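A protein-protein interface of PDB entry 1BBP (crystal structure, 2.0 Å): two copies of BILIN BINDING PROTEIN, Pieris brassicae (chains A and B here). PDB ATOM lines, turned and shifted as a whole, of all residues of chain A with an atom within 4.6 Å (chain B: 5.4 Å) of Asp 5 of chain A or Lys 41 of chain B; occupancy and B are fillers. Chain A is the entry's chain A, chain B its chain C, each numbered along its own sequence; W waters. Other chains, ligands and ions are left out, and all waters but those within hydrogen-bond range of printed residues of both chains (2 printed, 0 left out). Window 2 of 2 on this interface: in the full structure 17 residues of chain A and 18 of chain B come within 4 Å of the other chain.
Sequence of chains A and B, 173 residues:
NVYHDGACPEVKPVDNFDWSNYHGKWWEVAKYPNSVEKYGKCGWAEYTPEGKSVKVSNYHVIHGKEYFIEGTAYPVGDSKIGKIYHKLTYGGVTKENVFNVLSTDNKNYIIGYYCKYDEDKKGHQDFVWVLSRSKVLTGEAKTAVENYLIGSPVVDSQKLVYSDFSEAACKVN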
ATOM      1  N   HIS A   4     -25.419  11.220  21.180  1.00  0.00           N
ATOM      2  CA  HIS A   4     -24.449  10.530  22.051  1.00  0.00           C
ATOM      3  C   HIS A   4     -23.336   9.884  21.234  1.00  0.00           C
ATOM      4  O   HIS A   4     -23.566   9.466  20.103  1.00  0.00           O
ATOM      5  CB  HIS A   4     -25.068   9.414  22.900  1.00  0.00           C
ATOM      6  CG  HIS A   4     -26.070   9.941  23.941  1.00  0.00           C
ATOM      7  ND1 HIS A   4     -27.443  10.029  23.638  1.00  0.00           N
ATOM      8  CD2 HIS A   4     -25.852  10.386  25.200  1.00  0.00           C
ATOM      9  CE1 HIS A   4     -28.083  10.561  24.779  1.00  0.00           C
ATOM     10  NE2 HIS A   4     -27.092  10.786  25.755  1.00  0.00           N
ATOM     11  N   ASP A   5     -22.259   9.575  21.915  1.00  0.00           N
ATOM     12  CA  ASP A   5     -21.209   8.748  21.322  1.00  0.00           C
ATOM     13  C   ASP A   5     -21.651   7.287  21.332  1.00  0.00           C
ATOM     14  O   ASP A   5     -22.251   6.810  22.295  1.00  0.00           O
ATOM     15  CB  ASP A   5     -19.929   8.908  22.159  1.00  0.00           C
ATOM     16  CG  ASP A   5     -18.702   8.309  21.474  1.00  0.00           C
ATOM     17  OD1 ASP A   5     -17.743   7.960  22.209  1.00  0.00           O
ATOM     18  OD2 ASP A   5     -18.674   8.192  20.222  1.00  0.00           O
ATOM     19  N   GLY A   6     -21.242   6.594  20.305  1.00  0.00           N
ATOM     20  CA  GLY A   6     -21.327   5.135  20.332  1.00  0.00           C
ATOM     21  C   GLY A   6     -22.512   4.588  19.555  1.00  0.00           C
ATOM     22  O   GLY A   6     -23.183   5.311  18.828  1.00  0.00           O
ATOM     23  N   ALA A   7     -22.666   3.307  19.661  1.00  0.00           N
ATOM     24  CA  ALA A   7     -23.758   2.646  18.968  1.00  0.00           C
ATOM     25  C   ALA A   7     -25.059   2.900  19.720  1.00  0.00           C
ATOM     26  O   ALA A   7     -25.025   3.155  20.925  1.00  0.00           O
ATOM     27  CB  ALA A   7     -23.502   1.125  18.895  1.00  0.00           C
ATOM     28  N   LYS A 122     -19.451   7.538  14.118  1.00  0.00           N
ATOM     29  CA  LYS A 122     -19.624   6.571  15.203  1.00  0.00           C
ATOM     30  C   LYS A 122     -20.388   7.106  16.417  1.00  0.00           C
ATOM     31  O   LYS A 122     -20.046   6.833  17.569  1.00  0.00           O
ATOM     32  CB  LYS A 122     -18.259   5.941  15.538  1.00  0.00           C
ATOM     33  CG  LYS A 122     -17.714   5.313  14.357  1.00  0.00           C
ATOM     34  CD  LYS A 122     -17.006   4.059  14.682  1.00  0.00           C
ATOM     35  CE  LYS A 122     -15.862   3.783  13.244  1.00  0.00           C
ATOM     36  NZ  LYS A 122     -15.528   2.423  13.731  1.00  0.00           N
ATOM     37  N   GLY A 123     -21.511   7.748  16.124  1.00  0.00           N
ATOM     38  CA  GLY A 123     -22.401   8.238  17.195  1.00  0.00           C
ATOM     39  C   GLY A 123     -23.855   7.935  16.882  1.00  0.00           C
ATOM     40  O   GLY A 123     -24.167   7.540  15.769  1.00  0.00           O
ATOM     41  N   HIS A 124     -24.729   8.387  17.724  1.00  0.00           N
ATOM     42  CA  HIS A 124     -26.143   8.297  17.407  1.00  0.00           C
ATOM     43  C   HIS A 124     -26.998   9.404  18.028  1.00  0.00           C
ATOM     44  O   HIS A 124     -26.667   9.937  19.089  1.00  0.00           O
ATOM     45  CB  HIS A 124     -26.658   6.908  17.827  1.00  0.00           C
ATOM     46  CG  HIS A 124     -26.623   6.699  19.351  1.00  0.00           C
ATOM     47  ND1 HIS A 124     -25.523   6.141  20.007  1.00  0.00           N
ATOM     48  CD2 HIS A 124     -27.557   7.014  20.261  1.00  0.00           C
ATOM     49  CE1 HIS A 124     -25.827   6.136  21.372  1.00  0.00           C
ATOM     50  NE2 HIS A 124     -27.099   6.693  21.515  1.00  0.00           N
ATOM     51  N   TYR B  39     -21.281  14.920  17.686  1.00  0.00           N
ATOM     52  CA  TYR B  39     -20.346  13.822  17.960  1.00  0.00           C
ATOM     53  C   TYR B  39     -18.890  14.286  18.081  1.00  0.00           C
ATOM     54  O   TYR B  39     -18.021  13.475  18.421  1.00  0.00           O
ATOM     55  CB  TYR B  39     -20.433  12.685  16.912  1.00  0.00           C
ATOM     56  CG  TYR B  39     -21.873  12.225  16.617  1.00  0.00           C
ATOM     57  CD1 TYR B  39     -22.795  12.157  17.637  1.00  0.00           C
ATOM     58  CD2 TYR B  39     -22.256  11.958  15.320  1.00  0.00           C
ATOM     59  CE1 TYR B  39     -24.113  11.838  17.359  1.00  0.00           C
ATOM     60  CE2 TYR B  39     -23.570  11.643  15.037  1.00  0.00           C
ATOM     61  CZ  TYR B  39     -24.500  11.595  16.070  1.00  0.00           C
ATOM     62  OH  TYR B  39     -25.795  11.277  15.821  1.00  0.00           O
ATOM     63  N   GLY B  40     -18.632  15.559  17.820  1.00  0.00           N
ATOM     64  CA  GLY B  40     -17.240  16.049  17.909  1.00  0.00           C
ATOM     65  C   GLY B  40     -16.716  16.185  19.340  1.00  0.00           C
ATOM     66  O   GLY B  40     -17.477  16.449  20.266  1.00  0.00           O
ATOM     67  N   LYS B  41     -15.442  15.920  19.520  1.00  0.00           N
ATOM     68  CA  LYS B  41     -14.790  16.085  20.836  1.00  0.00           C
ATOM     69  C   LYS B  41     -13.622  17.060  20.715  1.00  0.00           C
ATOM     70  O   LYS B  41     -13.115  17.246  19.612  1.00  0.00           O
ATOM     71  CB  LYS B  41     -14.235  14.740  21.347  1.00  0.00           C
ATOM     72  CG  LYS B  41     -15.354  13.757  21.726  1.00  0.00           C
ATOM     73  CD  LYS B  41     -14.822  12.335  21.902  1.00  0.00           C
ATOM     74  CE  LYS B  41     -15.936  11.345  22.298  1.00  0.00           C
ATOM     75  NZ  LYS B  41     -16.343  11.595  23.682  1.00  0.00           N
ATOM     76  N   CYS B  42     -13.193  17.581  21.833  1.00  0.00           N
ATOM     77  CA  CYS B  42     -11.969  18.389  21.898  1.00  0.00           C
ATOM     78  C   CYS B  42     -11.972  19.583  20.951  1.00  0.00           C
ATOM     79  O   CYS B  42     -11.004  19.782  20.228  1.00  0.00           O
ATOM     80  CB  CYS B  42     -10.734  17.479  21.622  1.00  0.00           C
ATOM     81  SG  CYS B  42      -9.114  18.164  22.048  1.00  0.00           S
ATOM     82  N   GLY B  43     -13.047  20.332  20.895  1.00  0.00           N
ATOM     83  CA  GLY B  43     -13.111  21.431  19.924  1.00  0.00           C
ATOM     84  C   GLY B  43     -12.222  22.629  20.274  1.00  0.00           C
ATOM     85  O   GLY B  43     -12.073  22.996  21.433  1.00  0.00           O
ATOM     86  N   HIS B  60     -12.603  20.180  15.485  1.00  0.00           N
ATOM     87  CA  HIS B  60     -12.835  19.173  16.514  1.00  0.00           C
ATOM     88  C   HIS B  60     -12.258  17.836  16.070  1.00  0.00           C
ATOM     89  O   HIS B  60     -11.725  17.725  14.969  1.00  0.00           O
ATOM     90  CB  HIS B  60     -14.309  19.042  16.969  1.00  0.00           C
ATOM     91  CG  HIS B  60     -15.309  18.473  15.938  1.00  0.00           C
ATOM     92  ND1 HIS B  60     -16.613  18.980  15.877  1.00  0.00           N
ATOM     93  CD2 HIS B  60     -15.185  17.511  15.008  1.00  0.00           C
ATOM     94  CE1 HIS B  60     -17.284  18.311  14.847  1.00  0.00           C
ATOM     95  NE2 HIS B  60     -16.383  17.398  14.313  1.00  0.00           N
ATOM     96  N   VAL B  61     -12.357  16.867  16.935  1.00  0.00           N
ATOM     97  CA  VAL B  61     -11.820  15.552  16.634  1.00  0.00           C
ATOM     98  C   VAL B  61     -12.940  14.525  16.796  1.00  0.00           C
ATOM     99  O   VAL B  61     -13.618  14.492  17.816  1.00  0.00           O
ATOM    100  CB  VAL B  61     -10.623  15.231  17.582  1.00  0.00           C
ATOM    101  CG1 VAL B  61      -9.946  13.895  17.212  1.00  0.00           C
ATOM    102  CG2 VAL B  61      -9.564  16.357  17.587  1.00  0.00           C
ATOM    103  N   ILE B  62     -13.094  13.684  15.823  1.00  0.00           N
ATOM    104  CA  ILE B  62     -14.005  12.551  15.961  1.00  0.00           C
ATOM    105  C   ILE B  62     -13.202  11.297  15.608  1.00  0.00           C
ATOM    106  O   ILE B  62     -12.777  11.170  14.459  1.00  0.00           O
ATOM    107  CB  ILE B  62     -15.230  12.692  15.008  1.00  0.00           C
ATOM    108  CG1 ILE B  62     -16.091  13.943  15.283  1.00  0.00           C
ATOM    109  CG2 ILE B  62     -16.101  11.419  14.924  1.00  0.00           C
ATOM    110  CD1 ILE B  62     -17.260  14.100  14.272  1.00  0.00           C
ATOM    111  N   HIS B  63     -13.067  10.406  16.585  1.00  0.00           N
ATOM    112  CA  HIS B  63     -12.405   9.091  16.424  1.00  0.00           C
ATOM    113  C   HIS B  63     -11.107   9.169  15.625  1.00  0.00           C
ATOM    114  O   HIS B  63     -10.969   8.500  14.611  1.00  0.00           O
ATOM    115  CB  HIS B  63     -13.379   8.028  15.862  1.00  0.00           C
ATOM    116  CG  HIS B  63     -14.507   7.802  16.885  1.00  0.00           C
ATOM    117  ND1 HIS B  63     -14.267   7.091  18.074  1.00  0.00           N
ATOM    118  CD2 HIS B  63     -15.766   8.279  16.906  1.00  0.00           C
ATOM    119  CE1 HIS B  63     -15.437   7.144  18.861  1.00  0.00           C
ATOM    120  NE2 HIS B  63     -16.393   7.893  18.124  1.00  0.00           N
ATOM    121  N   ASP B 164     -15.270  17.280  25.864  1.00  0.00           N
ATOM    122  CA  ASP B 164     -14.345  16.258  26.315  1.00  0.00           C
ATOM    123  C   ASP B 164     -12.940  16.581  25.818  1.00  0.00           C
ATOM    124  O   ASP B 164     -12.669  16.476  24.615  1.00  0.00           O
ATOM    125  CB  ASP B 164     -14.848  14.899  25.798  1.00  0.00           C
ATOM    126  CG  ASP B 164     -14.050  13.746  26.393  1.00  0.00           C
ATOM    127  OD1 ASP B 164     -14.334  12.588  25.991  1.00  0.00           O
ATOM    128  OD2 ASP B 164     -13.156  13.976  27.249  1.00  0.00           O
ATOM    129  N   ALA B 169      -9.696  11.690  23.682  1.00  0.00           N
ATOM    130  CA  ALA B 169     -10.654  12.499  22.919  1.00  0.00           C
ATOM    131  C   ALA B 169      -9.919  13.351  21.885  1.00  0.00           C
ATOM    132  O   ALA B 169     -10.442  13.609  20.801  1.00  0.00           O
ATOM    133  CB  ALA B 169     -11.428  13.439  23.865  1.00  0.00           C
HETATM  134  O   HOH W   1     -18.956   9.704  17.991  1.00  0.00           O
HETATM  135  O   HOH W   2     -17.940   5.201  18.901  1.00  0.00           O
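The side-chain carboxylate (OD2) of Asp 5 of chain A is in hydrogen-bond range of a ring nitrogen (NE2) of His 63 of chain B (3.1 Å).
Of chain A, only Asp 5 (3.8 Å) comes within 4 Å of Lys 41 of chain B.
Printed residues of chain A within 4 Å of His 63 of chain B: Asp 5 and Lys 122.
Of the printed residues of chain B, Gly 123 of chain A touches Tyr 39 (3.8 Å).
Of the printed residues of chain A, Tyr 39 of chain B touches His 4, Gly 123 and His 124.
Of the printed residues of chain B, Lys 122 of chain A touches His 63.
Ala 7 of chain A touches none of the printed residues of chain B.
The nearest printed residue of chain A that does not touch Lys 41 of chain B is Gly 6 of chain A (7.4 Å).
No position is printed for both chains.
Of the 6 pairs that touch across the chains among the printed residues, none has its exchanged pair printed and touching as well.
Water W1 lies within hydrogen-bond range of the side-chain carboxylate of Asp 5 of chain A, the backbone carbonyl oxygen of Lys 122 of chain A and a ring nitrogen (NE2) of His 63 of chain B.
Water W2 lies within hydrogen-bond range of O of Lys 122 of chain A (3.0 Å), NE2 of His 63 of chain B (3.2 Å) and OD2 of Asp 5 of chain A (3.4 Å).
Of the 7 printed residues of chain A, 5 touch a printed residue of chain B.
Of the 11 printed residues of chain B, 3 touch a printed residue of chain A.
Hydrophobic or aromatic side chains of chain B within 4 Å of the printed part of chain A: Tyr 39 and His 63.
Among the printed residues, 6 pairs touch across the chains.
Among the printed residues, no Asp or Glu carboxylate lies within 4 Å of a Lys or Arg side-chain nitrogen of the other chain.
O of His 124 of chain A is in hydrogen-bond range of N of His 4 of chain A (2.8 Å).
The backbone NH (N) of Gly 6 of chain A lies within hydrogen-bond range of the backbone carbonyl oxygen (O) of Lys 122 of chain A (3.0 Å).
O of Gly 6 of chain A lies within hydrogen-bond range of ND1 of His 124 of chain A, 2.7 Å away.
The backbone carbonyl oxygen (O) of Ala 7 of chain A sits close to a ring nitrogen (ND1) of His 124 of chain A (3.2 Å).
The backbone carbonyl oxygen of Lys 41 of chain B sits at hydrogen-bond distance from the backbone NH of Val 61 of chain B (2.8 Å).
The side-chain carboxylate (OD1) of Asp 164 of chain B lies within salt-bridge range of the side-chain amino group (NZ) of Lys 41 of chain B (3.2 Å).
O of His 4 of chain A touches CE1 of Tyr 39 of chain B, at 3.7 Å.
OD1 of Asp 5 of chain A touches CE of Lys 41 of chain B (3.8 Å).
Lys 122 of chain A touches His 63 of chain B.
Tyr 39 of chain B touches Gly 123 of chain A (CZ to C, 3.8 Å).
His 124 of chain A touches Tyr 39 of chain B (C to OH, 3.1 Å).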
